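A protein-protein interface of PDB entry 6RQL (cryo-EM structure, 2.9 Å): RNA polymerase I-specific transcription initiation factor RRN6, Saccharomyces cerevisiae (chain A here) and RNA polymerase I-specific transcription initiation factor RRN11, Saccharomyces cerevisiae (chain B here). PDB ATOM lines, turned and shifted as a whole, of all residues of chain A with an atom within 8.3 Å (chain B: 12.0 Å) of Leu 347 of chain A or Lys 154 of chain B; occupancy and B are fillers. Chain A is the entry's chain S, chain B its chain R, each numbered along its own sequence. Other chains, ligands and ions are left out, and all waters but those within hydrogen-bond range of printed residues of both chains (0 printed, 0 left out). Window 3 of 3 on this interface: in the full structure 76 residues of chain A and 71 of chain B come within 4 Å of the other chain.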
ATOM      1  N   ALA A 316       6.197 -18.154  25.379  1.00  0.00           N
ATOM      2  CA  ALA A 316       5.990 -17.103  26.366  1.00  0.00           C
ATOM      3  C   ALA A 316       4.565 -17.130  26.899  1.00  0.00           C
ATOM      4  O   ALA A 316       3.759 -16.267  26.574  1.00  0.00           O
ATOM      5  CB  ALA A 316       6.304 -15.748  25.769  1.00  0.00           C
ATOM      6  N   ASN A 323      -5.099 -11.718  34.483  1.00  0.00           N
ATOM      7  CA  ASN A 323      -5.238 -12.044  33.071  1.00  0.00           C
ATOM      8  C   ASN A 323      -3.990 -12.732  32.531  1.00  0.00           C
ATOM      9  O   ASN A 323      -2.865 -12.443  32.939  1.00  0.00           O
ATOM     10  CB  ASN A 323      -5.573 -10.793  32.245  1.00  0.00           C
ATOM     11  CG  ASN A 323      -4.674  -9.621  32.558  1.00  0.00           C
ATOM     12  OD1 ASN A 323      -3.760  -9.724  33.366  1.00  0.00           O
ATOM     13  ND2 ASN A 323      -4.946  -8.487  31.927  1.00  0.00           N
ATOM     14  N   TRP A 324      -4.215 -13.648  31.597  1.00  0.00           N
ATOM     15  CA  TRP A 324      -3.201 -14.528  31.039  1.00  0.00           C
ATOM     16  C   TRP A 324      -3.005 -14.204  29.567  1.00  0.00           C
ATOM     17  O   TRP A 324      -3.833 -13.543  28.934  1.00  0.00           O
ATOM     18  CB  TRP A 324      -3.605 -15.997  31.214  1.00  0.00           C
ATOM     19  CG  TRP A 324      -4.918 -16.333  30.571  1.00  0.00           C
ATOM     20  CD1 TRP A 324      -6.155 -16.110  31.090  1.00  0.00           C
ATOM     21  CD2 TRP A 324      -5.126 -16.994  29.320  1.00  0.00           C
ATOM     22  NE1 TRP A 324      -7.120 -16.561  30.229  1.00  0.00           N
ATOM     23  CE2 TRP A 324      -6.513 -17.108  29.133  1.00  0.00           C
ATOM     24  CE3 TRP A 324      -4.275 -17.487  28.330  1.00  0.00           C
ATOM     25  CZ2 TRP A 324      -7.064 -17.694  28.006  1.00  0.00           C
ATOM     26  CZ3 TRP A 324      -4.829 -18.071  27.214  1.00  0.00           C
ATOM     27  CH2 TRP A 324      -6.207 -18.171  27.062  1.00  0.00           C
ATOM     28  N   SER A 325      -1.888 -14.674  29.019  1.00  0.00           N
ATOM     29  CA  SER A 325      -1.594 -14.427  27.617  1.00  0.00           C
ATOM     30  C   SER A 325      -0.700 -15.533  27.084  1.00  0.00           C
ATOM     31  O   SER A 325      -0.072 -16.276  27.843  1.00  0.00           O
ATOM     32  CB  SER A 325      -0.936 -13.060  27.413  1.00  0.00           C
ATOM     33  OG  SER A 325      -1.837 -12.015  27.727  1.00  0.00           O
ATOM     34  N   ILE A 326      -0.661 -15.629  25.759  1.00  0.00           N
ATOM     35  CA  ILE A 326       0.125 -16.623  25.044  1.00  0.00           C
ATOM     36  C   ILE A 326       1.141 -15.870  24.199  1.00  0.00           C
ATOM     37  O   ILE A 326       0.818 -14.824  23.630  1.00  0.00           O
ATOM     38  CB  ILE A 326      -0.770 -17.520  24.173  1.00  0.00           C
ATOM     39  CG1 ILE A 326      -1.914 -18.082  25.011  1.00  0.00           C
ATOM     40  CG2 ILE A 326       0.024 -18.679  23.594  1.00  0.00           C
ATOM     41  CD1 ILE A 326      -1.463 -18.930  26.175  1.00  0.00           C
ATOM     42  N   GLY A 327       2.369 -16.370  24.151  1.00  0.00           N
ATOM     43  CA  GLY A 327       3.440 -15.748  23.387  1.00  0.00           C
ATOM     44  C   GLY A 327       4.055 -16.731  22.408  1.00  0.00           C
ATOM     45  O   GLY A 327       3.876 -17.945  22.538  1.00  0.00           O
ATOM     46  N   ARG A 328       4.776 -16.196  21.430  1.00  0.00           N
ATOM     47  CA  ARG A 328       5.426 -16.998  20.398  1.00  0.00           C
ATOM     48  C   ARG A 328       6.930 -16.872  20.603  1.00  0.00           C
ATOM     49  O   ARG A 328       7.492 -15.778  20.510  1.00  0.00           O
ATOM     50  CB  ARG A 328       4.999 -16.533  19.012  1.00  0.00           C
ATOM     51  CG  ARG A 328       5.444 -17.434  17.894  1.00  0.00           C
ATOM     52  CD  ARG A 328       5.021 -16.868  16.554  1.00  0.00           C
ATOM     53  NE  ARG A 328       3.575 -16.863  16.360  1.00  0.00           N
ATOM     54  CZ  ARG A 328       2.884 -17.895  15.885  1.00  0.00           C
ATOM     55  NH1 ARG A 328       3.509 -19.017  15.562  1.00  0.00           N
ATOM     56  NH2 ARG A 328       1.569 -17.807  15.732  1.00  0.00           N
ATOM     57  N   ILE A 344       4.200 -11.429  22.493  1.00  0.00           N
ATOM     58  CA  ILE A 344       2.914 -11.973  22.912  1.00  0.00           C
ATOM     59  C   ILE A 344       2.028 -12.174  21.690  1.00  0.00           C
ATOM     60  O   ILE A 344       1.932 -11.294  20.826  1.00  0.00           O
ATOM     61  CB  ILE A 344       2.253 -11.041  23.941  1.00  0.00           C
ATOM     62  CG1 ILE A 344       3.189 -10.813  25.126  1.00  0.00           C
ATOM     63  CG2 ILE A 344       0.941 -11.613  24.451  1.00  0.00           C
ATOM     64  CD1 ILE A 344       3.538 -12.073  25.871  1.00  0.00           C
ATOM     65  N   ASP A 345       1.381 -13.336  21.610  1.00  0.00           N
ATOM     66  CA  ASP A 345       0.417 -13.620  20.559  1.00  0.00           C
ATOM     67  C   ASP A 345      -0.890 -12.878  20.857  1.00  0.00           C
ATOM     68  O   ASP A 345      -1.107 -12.367  21.957  1.00  0.00           O
ATOM     69  CB  ASP A 345       0.215 -15.134  20.447  1.00  0.00           C
ATOM     70  CG  ASP A 345      -0.418 -15.559  19.146  1.00  0.00           C
ATOM     71  OD1 ASP A 345      -0.795 -14.686  18.342  1.00  0.00           O
ATOM     72  OD2 ASP A 345      -0.522 -16.779  18.917  1.00  0.00           O
ATOM     73  N   ASN A 346      -1.776 -12.824  19.861  1.00  0.00           N
ATOM     74  CA  ASN A 346      -2.954 -11.962  19.899  1.00  0.00           C
ATOM     75  C   ASN A 346      -4.208 -12.682  20.383  1.00  0.00           C
ATOM     76  O   ASN A 346      -5.299 -12.456  19.841  1.00  0.00           O
ATOM     77  CB  ASN A 346      -3.189 -11.336  18.526  1.00  0.00           C
ATOM     78  CG  ASN A 346      -2.162 -10.276  18.194  1.00  0.00           C
ATOM     79  OD1 ASN A 346      -1.813  -9.453  19.039  1.00  0.00           O
ATOM     80  ND2 ASN A 346      -1.665 -10.293  16.963  1.00  0.00           N
ATOM     81  N   LEU A 347      -4.074 -13.568  21.366  1.00  0.00           N
ATOM     82  CA  LEU A 347      -5.202 -14.257  21.978  1.00  0.00           C
ATOM     83  C   LEU A 347      -4.917 -14.408  23.464  1.00  0.00           C
ATOM     84  O   LEU A 347      -3.781 -14.698  23.853  1.00  0.00           O
ATOM     85  CB  LEU A 347      -5.445 -15.604  21.283  1.00  0.00           C
ATOM     86  CG  LEU A 347      -4.299 -16.615  21.167  1.00  0.00           C
ATOM     87  CD1 LEU A 347      -4.331 -17.648  22.276  1.00  0.00           C
ATOM     88  CD2 LEU A 347      -4.286 -17.282  19.800  1.00  0.00           C
ATOM     89  N   HIS A 348      -5.935 -14.193  24.289  1.00  0.00           N
ATOM     90  CA  HIS A 348      -5.721 -13.938  25.708  1.00  0.00           C
ATOM     91  C   HIS A 348      -7.031 -14.166  26.455  1.00  0.00           C
ATOM     92  O   HIS A 348      -8.011 -14.666  25.894  1.00  0.00           O
ATOM     93  CB  HIS A 348      -5.233 -12.505  25.919  1.00  0.00           C
ATOM     94  CG  HIS A 348      -6.277 -11.484  25.600  1.00  0.00           C
ATOM     95  ND1 HIS A 348      -6.590 -11.123  24.308  1.00  0.00           N
ATOM     96  CD2 HIS A 348      -7.110 -10.779  26.401  1.00  0.00           C
ATOM     97  CE1 HIS A 348      -7.560 -10.227  24.329  1.00  0.00           C
ATOM     98  NE2 HIS A 348      -7.891  -9.998  25.586  1.00  0.00           N
ATOM     99  N   GLY A 349      -7.050 -13.762  27.718  1.00  0.00           N
ATOM    100  CA  GLY A 349      -8.239 -13.862  28.537  1.00  0.00           C
ATOM    101  C   GLY A 349      -7.906 -13.490  29.968  1.00  0.00           C
ATOM    102  O   GLY A 349      -6.772 -13.125  30.280  1.00  0.00           O
ATOM    103  N   THR A 350      -8.906 -13.616  30.836  1.00  0.00           N
ATOM    104  CA  THR A 350      -8.741 -13.227  32.227  1.00  0.00           C
ATOM    105  C   THR A 350      -9.544 -14.146  33.132  1.00  0.00           C
ATOM    106  O   THR A 350     -10.468 -14.836  32.697  1.00  0.00           O
ATOM    107  CB  THR A 350      -9.167 -11.775  32.467  1.00  0.00           C
ATOM    108  OG1 THR A 350      -8.891 -11.419  33.826  1.00  0.00           O
ATOM    109  CG2 THR A 350     -10.647 -11.595  32.196  1.00  0.00           C
ATOM    110  N   ILE A 372      -4.923 -25.272  28.893  1.00  0.00           N
ATOM    111  CA  ILE A 372      -4.188 -24.736  30.023  1.00  0.00           C
ATOM    112  C   ILE A 372      -5.075 -24.760  31.262  1.00  0.00           C
ATOM    113  O   ILE A 372      -6.305 -24.843  31.185  1.00  0.00           O
ATOM    114  CB  ILE A 372      -3.683 -23.312  29.730  1.00  0.00           C
ATOM    115  CG1 ILE A 372      -4.850 -22.349  29.583  1.00  0.00           C
ATOM    116  CG2 ILE A 372      -2.919 -23.287  28.443  1.00  0.00           C
ATOM    117  CD1 ILE A 372      -4.410 -20.920  29.479  1.00  0.00           C
ATOM    118  N   ILE A 383      -9.199 -23.742  30.512  1.00  0.00           N
ATOM    119  CA  ILE A 383      -9.395 -22.916  29.330  1.00  0.00           C
ATOM    120  C   ILE A 383      -8.767 -23.612  28.135  1.00  0.00           C
ATOM    121  O   ILE A 383      -7.561 -23.879  28.136  1.00  0.00           O
ATOM    122  CB  ILE A 383      -8.768 -21.523  29.495  1.00  0.00           C
ATOM    123  CG1 ILE A 383      -9.374 -20.784  30.674  1.00  0.00           C
ATOM    124  CG2 ILE A 383      -8.992 -20.723  28.250  1.00  0.00           C
ATOM    125  CD1 ILE A 383      -8.608 -19.550  31.056  1.00  0.00           C
ATOM    126  N   ASP A 384      -9.571 -23.884  27.110  1.00  0.00           N
ATOM    127  CA  ASP A 384      -9.056 -24.189  25.780  1.00  0.00           C
ATOM    128  C   ASP A 384      -9.009 -22.881  25.002  1.00  0.00           C
ATOM    129  O   ASP A 384     -10.053 -22.321  24.654  1.00  0.00           O
ATOM    130  CB  ASP A 384      -9.911 -25.218  25.047  1.00  0.00           C
ATOM    131  CG  ASP A 384      -9.318 -25.611  23.700  1.00  0.00           C
ATOM    132  OD1 ASP A 384      -8.348 -26.399  23.669  1.00  0.00           O
ATOM    133  OD2 ASP A 384      -9.811 -25.116  22.663  1.00  0.00           O
ATOM    134  N   PHE A 385      -7.804 -22.386  24.747  1.00  0.00           N
ATOM    135  CA  PHE A 385      -7.648 -21.194  23.930  1.00  0.00           C
ATOM    136  C   PHE A 385      -7.788 -21.484  22.446  1.00  0.00           C
ATOM    137  O   PHE A 385      -7.896 -20.541  21.653  1.00  0.00           O
ATOM    138  CB  PHE A 385      -6.297 -20.517  24.218  1.00  0.00           C
ATOM    139  CG  PHE A 385      -5.096 -21.386  23.949  1.00  0.00           C
ATOM    140  CD1 PHE A 385      -4.592 -22.219  24.933  1.00  0.00           C
ATOM    141  CD2 PHE A 385      -4.447 -21.338  22.729  1.00  0.00           C
ATOM    142  CE1 PHE A 385      -3.496 -23.002  24.699  1.00  0.00           C
ATOM    143  CE2 PHE A 385      -3.348 -22.127  22.491  1.00  0.00           C
ATOM    144  CZ  PHE A 385      -2.875 -22.956  23.484  1.00  0.00           C
ATOM    145  N   MET A 386      -7.788 -22.755  22.052  1.00  0.00           N
ATOM    146  CA  MET A 386      -7.925 -23.082  20.644  1.00  0.00           C
ATOM    147  C   MET A 386      -9.369 -22.937  20.184  1.00  0.00           C
ATOM    148  O   MET A 386      -9.615 -22.543  19.039  1.00  0.00           O
ATOM    149  CB  MET A 386      -7.402 -24.495  20.390  1.00  0.00           C
ATOM    150  CG  MET A 386      -7.130 -24.783  18.942  1.00  0.00           C
ATOM    151  SD  MET A 386      -5.890 -23.618  18.354  1.00  0.00           S
ATOM    152  CE  MET A 386      -4.465 -24.159  19.289  1.00  0.00           C
ATOM    153  N   ASN A 387     -10.322 -23.241  21.053  1.00  0.00           N
ATOM    154  CA  ASN A 387     -11.724 -22.932  20.855  1.00  0.00           C
ATOM    155  C   ASN A 387     -12.094 -21.740  21.730  1.00  0.00           C
ATOM    156  O   ASN A 387     -11.231 -21.063  22.292  1.00  0.00           O
ATOM    157  CB  ASN A 387     -12.573 -24.157  21.168  1.00  0.00           C
ATOM    158  CG  ASN A 387     -12.343 -25.271  20.189  1.00  0.00           C
ATOM    159  OD1 ASN A 387     -12.297 -25.044  18.986  1.00  0.00           O
ATOM    160  ND2 ASN A 387     -12.166 -26.482  20.696  1.00  0.00           N
ATOM    161  N   ASN A 388     -13.384 -21.456  21.832  1.00  0.00           N
ATOM    162  CA  ASN A 388     -13.903 -20.579  22.873  1.00  0.00           C
ATOM    163  C   ASN A 388     -14.503 -21.460  23.961  1.00  0.00           C
ATOM    164  O   ASN A 388     -15.693 -21.790  23.913  1.00  0.00           O
ATOM    165  CB  ASN A 388     -14.932 -19.592  22.328  1.00  0.00           C
ATOM    166  CG  ASN A 388     -14.294 -18.445  21.570  1.00  0.00           C
ATOM    167  OD1 ASN A 388     -13.235 -17.945  21.951  1.00  0.00           O
ATOM    168  ND2 ASN A 388     -14.957 -17.998  20.512  1.00  0.00           N
ATOM    169  N   GLN A 390     -14.186 -22.239  28.278  1.00  0.00           N
ATOM    170  CA  GLN A 390     -13.668 -21.875  29.592  1.00  0.00           C
ATOM    171  C   GLN A 390     -14.633 -22.402  30.638  1.00  0.00           C
ATOM    172  O   GLN A 390     -15.840 -22.192  30.517  1.00  0.00           O
ATOM    173  CB  GLN A 390     -13.533 -20.358  29.734  1.00  0.00           C
ATOM    174  CG  GLN A 390     -12.975 -19.924  31.056  1.00  0.00           C
ATOM    175  CD  GLN A 390     -12.958 -18.425  31.231  1.00  0.00           C
ATOM    176  OE1 GLN A 390     -13.477 -17.689  30.402  1.00  0.00           O
ATOM    177  NE2 GLN A 390     -12.352 -17.963  32.314  1.00  0.00           N
ATOM    178  N   PHE B  31     -17.808  -3.140  40.916  1.00  0.00           N
ATOM    179  CA  PHE B  31     -17.564  -3.887  39.688  1.00  0.00           C
ATOM    180  C   PHE B  31     -18.871  -4.317  39.031  1.00  0.00           C
ATOM    181  O   PHE B  31     -18.891  -4.613  37.832  1.00  0.00           O
ATOM    182  CB  PHE B  31     -16.683  -5.098  39.992  1.00  0.00           C
ATOM    183  CG  PHE B  31     -16.223  -5.842  38.776  1.00  0.00           C
ATOM    184  CD1 PHE B  31     -15.212  -5.334  37.982  1.00  0.00           C
ATOM    185  CD2 PHE B  31     -16.792  -7.057  38.434  1.00  0.00           C
ATOM    186  CE1 PHE B  31     -14.779  -6.015  36.868  1.00  0.00           C
ATOM    187  CE2 PHE B  31     -16.361  -7.747  37.315  1.00  0.00           C
ATOM    188  CZ  PHE B  31     -15.354  -7.223  36.534  1.00  0.00           C
ATOM    189  N   SER B  35     -18.755  -3.545  34.541  1.00  0.00           N
ATOM    190  CA  SER B  35     -18.917  -4.548  33.495  1.00  0.00           C
ATOM    191  C   SER B  35     -20.236  -4.384  32.751  1.00  0.00           C
ATOM    192  O   SER B  35     -20.355  -4.845  31.611  1.00  0.00           O
ATOM    193  CB  SER B  35     -18.816  -5.953  34.089  1.00  0.00           C
ATOM    194  OG  SER B  35     -18.931  -6.943  33.083  1.00  0.00           O
ATOM    195  N   SER B  38     -20.080  -1.788  29.517  1.00  0.00           N
ATOM    196  CA  SER B  38     -19.306  -2.165  28.340  1.00  0.00           C
ATOM    197  C   SER B  38     -19.639  -3.583  27.891  1.00  0.00           C
ATOM    198  O   SER B  38     -18.758  -4.335  27.480  1.00  0.00           O
ATOM    199  CB  SER B  38     -17.812  -2.044  28.630  1.00  0.00           C
ATOM    200  OG  SER B  38     -17.420  -2.964  29.633  1.00  0.00           O
ATOM    201  N   GLN B 150     -18.434 -22.244  28.790  1.00  0.00           N
ATOM    202  CA  GLN B 150     -18.533 -20.792  28.820  1.00  0.00           C
ATOM    203  C   GLN B 150     -17.397 -20.256  27.964  1.00  0.00           C
ATOM    204  O   GLN B 150     -16.307 -20.833  27.973  1.00  0.00           O
ATOM    205  CB  GLN B 150     -18.431 -20.270  30.264  1.00  0.00           C
ATOM    206  CG  GLN B 150     -18.852 -18.834  30.524  1.00  0.00           C
ATOM    207  CD  GLN B 150     -20.358 -18.655  30.496  1.00  0.00           C
ATOM    208  OE1 GLN B 150     -21.101 -19.538  30.922  1.00  0.00           O
ATOM    209  NE2 GLN B 150     -20.815 -17.498  30.032  1.00  0.00           N
ATOM    210  N   PRO B 151     -17.620 -19.205  27.184  1.00  0.00           N
ATOM    211  CA  PRO B 151     -16.539 -18.684  26.339  1.00  0.00           C
ATOM    212  C   PRO B 151     -15.527 -17.900  27.158  1.00  0.00           C
ATOM    213  O   PRO B 151     -15.771 -17.527  28.307  1.00  0.00           O
ATOM    214  CB  PRO B 151     -17.268 -17.778  25.341  1.00  0.00           C
ATOM    215  CG  PRO B 151     -18.692 -18.238  25.378  1.00  0.00           C
ATOM    216  CD  PRO B 151     -18.923 -18.643  26.802  1.00  0.00           C
ATOM    217  N   ILE B 152     -14.367 -17.653  26.545  1.00  0.00           N
ATOM    218  CA  ILE B 152     -13.331 -16.871  27.215  1.00  0.00           C
ATOM    219  C   ILE B 152     -13.747 -15.409  27.265  1.00  0.00           C
ATOM    220  O   ILE B 152     -13.961 -14.772  26.226  1.00  0.00           O
ATOM    221  CB  ILE B 152     -11.969 -17.020  26.518  1.00  0.00           C
ATOM    222  CG1 ILE B 152     -11.426 -18.438  26.643  1.00  0.00           C
ATOM    223  CG2 ILE B 152     -10.959 -16.064  27.118  1.00  0.00           C
ATOM    224  CD1 ILE B 152     -11.596 -19.276  25.437  1.00  0.00           C
ATOM    225  N   ASN B 153     -13.856 -14.867  28.476  1.00  0.00           N
ATOM    226  CA  ASN B 153     -14.131 -13.446  28.654  1.00  0.00           C
ATOM    227  C   ASN B 153     -12.859 -12.660  28.350  1.00  0.00           C
ATOM    228  O   ASN B 153     -12.042 -12.366  29.223  1.00  0.00           O
ATOM    229  CB  ASN B 153     -14.685 -13.167  30.048  1.00  0.00           C
ATOM    230  CG  ASN B 153     -13.875 -13.817  31.153  1.00  0.00           C
ATOM    231  OD1 ASN B 153     -12.897 -14.512  30.895  1.00  0.00           O
ATOM    232  ND2 ASN B 153     -14.264 -13.567  32.397  1.00  0.00           N
ATOM    233  N   LYS B 154     -12.703 -12.279  27.085  1.00  0.00           N
ATOM    234  CA  LYS B 154     -11.506 -11.576  26.647  1.00  0.00           C
ATOM    235  C   LYS B 154     -11.516 -10.092  27.015  1.00  0.00           C
ATOM    236  O   LYS B 154     -10.572  -9.377  26.663  1.00  0.00           O
ATOM    237  CB  LYS B 154     -11.320 -11.764  25.139  1.00  0.00           C
ATOM    238  CG  LYS B 154     -11.129 -13.229  24.776  1.00  0.00           C
ATOM    239  CD  LYS B 154     -10.869 -13.491  23.303  1.00  0.00           C
ATOM    240  CE  LYS B 154      -9.428 -13.165  22.942  1.00  0.00           C
ATOM    241  NZ  LYS B 154      -9.095 -13.569  21.548  1.00  0.00           N
ATOM    242  N   GLN B 155     -12.541  -9.622  27.723  1.00  0.00           N
ATOM    243  CA  GLN B 155     -12.576  -8.270  28.275  1.00  0.00           C
ATOM    244  C   GLN B 155     -11.754  -8.271  29.557  1.00  0.00           C
ATOM    245  O   GLN B 155     -12.273  -8.546  30.639  1.00  0.00           O
ATOM    246  CB  GLN B 155     -14.012  -7.836  28.540  1.00  0.00           C
ATOM    247  CG  GLN B 155     -14.869  -7.688  27.297  1.00  0.00           C
ATOM    248  CD  GLN B 155     -14.482  -6.488  26.461  1.00  0.00           C
ATOM    249  OE1 GLN B 155     -14.172  -5.423  26.992  1.00  0.00           O
ATOM    250  NE2 GLN B 155     -14.502  -6.651  25.147  1.00  0.00           N
ATOM    251  N   LYS B 156     -10.469  -7.950  29.437  1.00  0.00           N
ATOM    252  CA  LYS B 156      -9.546  -8.030  30.558  1.00  0.00           C
ATOM    253  C   LYS B 156      -9.647  -6.789  31.448  1.00  0.00           C
ATOM    254  O   LYS B 156     -10.453  -5.883  31.224  1.00  0.00           O
ATOM    255  CB  LYS B 156      -8.109  -8.179  30.062  1.00  0.00           C
ATOM    256  CG  LYS B 156      -7.598  -6.926  29.377  1.00  0.00           C
ATOM    257  CD  LYS B 156      -6.152  -7.036  28.984  1.00  0.00           C
ATOM    258  CE  LYS B 156      -5.686  -5.720  28.398  1.00  0.00           C
ATOM    259  NZ  LYS B 156      -6.387  -5.430  27.119  1.00  0.00           N
ATOM    260  N   MET B 157      -8.807  -6.767  32.482  1.00  0.00           N
ATOM    261  CA  MET B 157      -8.612  -5.591  33.320  1.00  0.00           C
ATOM    262  C   MET B 157      -7.214  -5.027  33.077  1.00  0.00           C
ATOM    263  O   MET B 157      -6.266  -5.788  32.859  1.00  0.00           O
ATOM    264  CB  MET B 157      -8.795  -5.943  34.794  1.00  0.00           C
ATOM    265  CG  MET B 157     -10.198  -6.339  35.162  1.00  0.00           C
ATOM    266  SD  MET B 157     -11.358  -5.019  34.798  1.00  0.00           S
ATOM    267  CE  MET B 157     -10.794  -3.768  35.941  1.00  0.00           C
ATOM    268  N   THR B 158      -7.089  -3.700  33.102  1.00  0.00           N
ATOM    269  CA  THR B 158      -5.787  -3.055  33.064  1.00  0.00           C
ATOM    270  C   THR B 158      -5.642  -2.081  34.232  1.00  0.00           C
ATOM    271  O   THR B 158      -6.546  -1.910  35.053  1.00  0.00           O
ATOM    272  CB  THR B 158      -5.563  -2.346  31.729  1.00  0.00           C
ATOM    273  OG1 THR B 158      -4.203  -1.906  31.655  1.00  0.00           O
ATOM    274  CG2 THR B 158      -6.481  -1.146  31.598  1.00  0.00           C
ATOM    275  N   ASN B 161      -8.124   0.989  34.758  1.00  0.00           N
ATOM    276  CA  ASN B 161      -9.440   0.571  35.212  1.00  0.00           C
ATOM    277  C   ASN B 161      -9.419   0.041  36.634  1.00  0.00           C
ATOM    278  O   ASN B 161     -10.457   0.057  37.301  1.00  0.00           O
ATOM    279  CB  ASN B 161     -10.006  -0.494  34.275  1.00  0.00           C
ATOM    280  CG  ASN B 161     -10.274   0.040  32.888  1.00  0.00           C
ATOM    281  OD1 ASN B 161      -9.674  -0.403  31.913  1.00  0.00           O
ATOM    282  ND2 ASN B 161     -11.174   1.010  32.795  1.00  0.00           N
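The backbone NH of Trp 324 of chain A sits at hydrogen-bond distance from the backbone carbonyl oxygen of Gly 349 of chain A, 2.9 Å away.
N of Ile 372 of chain A lies within hydrogen-bond range of O of Ile 383 of chain A (3.1 Å).
OD2 of Asp 384 of chain A lies within hydrogen-bond range of N of Met 386 of chain A, 3.2 Å away.
N of Asn 387 of chain A is in hydrogen-bond range of OD2 of Asp 384 of chain A (2.5 Å).
Among the printed residues, merely in contact across the chains: Gln 390 of chain A with Ile 152 of chain B, His 348 of chain A with Ile 152 of chain B, Asn 323 of chain A with Lys 156 of chain B, Asp 384 of chain A with Ile 152 of chain B, Asn 387 of chain A with Ile 152 of chain B, Asn 388 of chain A with Ile 152 of chain B, Ile 383 of chain A with Ile 152 of chain B, Gly 349 of chain A with Ile 152 of chain B, Thr 350 of chain A with Gln 155 of chain B and Leu 347 of chain A with Lys 154 of chain B.
The side-chain amide nitrogen (ND2) of Asn 323 of chain A sits at hydrogen-bond distance from the backbone carbonyl oxygen (O) of Met 157 of chain B (3.1 Å).
NE2 of His 348 of chain A sits at hydrogen-bond distance from O of Lys 154 of chain B (3.0 Å).
The side-chain amide oxygen of Asn 153 of chain B lies close to the backbone carbonyl oxygen of Thr 350 of chain A, 3.0 Å away.
The backbone NH of Gln 390 of chain A lies within hydrogen-bond range of the backbone carbonyl oxygen of Gln 150 of chain B (2.6 Å).
OE1 of Gln 390 of chain A lies close to O of Pro 151 of chain B, 3.1 Å away.
The side-chain amide oxygen of Gln 390 of chain A lies close to the side-chain amide oxygen of Asn 153 of chain B (3.3 Å).
Of the 13 printed residues of chain B, 8 touch a printed residue of chain A.
Printed residues of chain B that touch a printed residue of chain A: Gln 150, Pro 151, Ile 152, Asn 153, Lys 154, Gln 155, Lys 156 and Met 157.
Of the 22 printed residues of chain A, 10 touch a printed residue of chain B.
Printed residues of chain A that touch a printed residue of chain B: Asn 323, Leu 347, His 348, Gly 349, Thr 350, Ile 383, Asp 384, Asn 387, Asn 388 and Gln 390.
Hydrophobic or aromatic side chains of chain A that line the printed part of chain B: His 348 and Ile 383.
Among the printed residues, no Asp or Glu carboxylate lies within 4 Å of a Lys or Arg side-chain nitrogen of the other chain.
Leu 347 of chain A touches one residue of chain B.
Lys 154 of chain B touches just these residues of chain A: Leu 347 and His 348.
Trp 324 of chain A touches none of the printed residues of chain B.
No residue of chain B comes within 4 Å of Ser 325 of chain A.
No residue of chain B comes within 4 Å of Ile 326 of chain A.
No residue of chain B comes within 4 Å of Asp 345 of chain A.
No residue of chain B comes within 4 Å of Asn 346 of chain A.
His 348 of chain A touches just these residues of chain B: Ile 152 and Lys 154.
Of the printed residues of chain B, Gly 349 of chain A touches Ile 152 (3.8 Å).
Of chain B, only Asn 153 (3.0 Å) and Gln 155 (3.8 Å) come within 4 Å of Thr 350 of chain A.
Of the printed residues of chain B, Ile 383 of chain A touches Ile 152 (3.7 Å).
Printed residues of chain A within 4 Å of Gln 155 of chain B: Thr 350.
Printed residues of chain A within 4 Å of Met 157 of chain B: Asn 323 (3.1 Å).
Ala 316 of chain A touches none of the printed residues of chain B.
Arg 328 of chain A touches none of the printed residues of chain B.
The nearest residue of chain B that does not touch Leu 347 of chain A is Ile 152 of chain B (7.3 Å).
The nearest residue of chain A that does not touch Lys 154 of chain B is Asn 346 of chain A (4.3 Å).
The nearest printed residue of chain A that does not touch Ile 152 of chain B is Trp 324 of chain A (4.3 Å).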
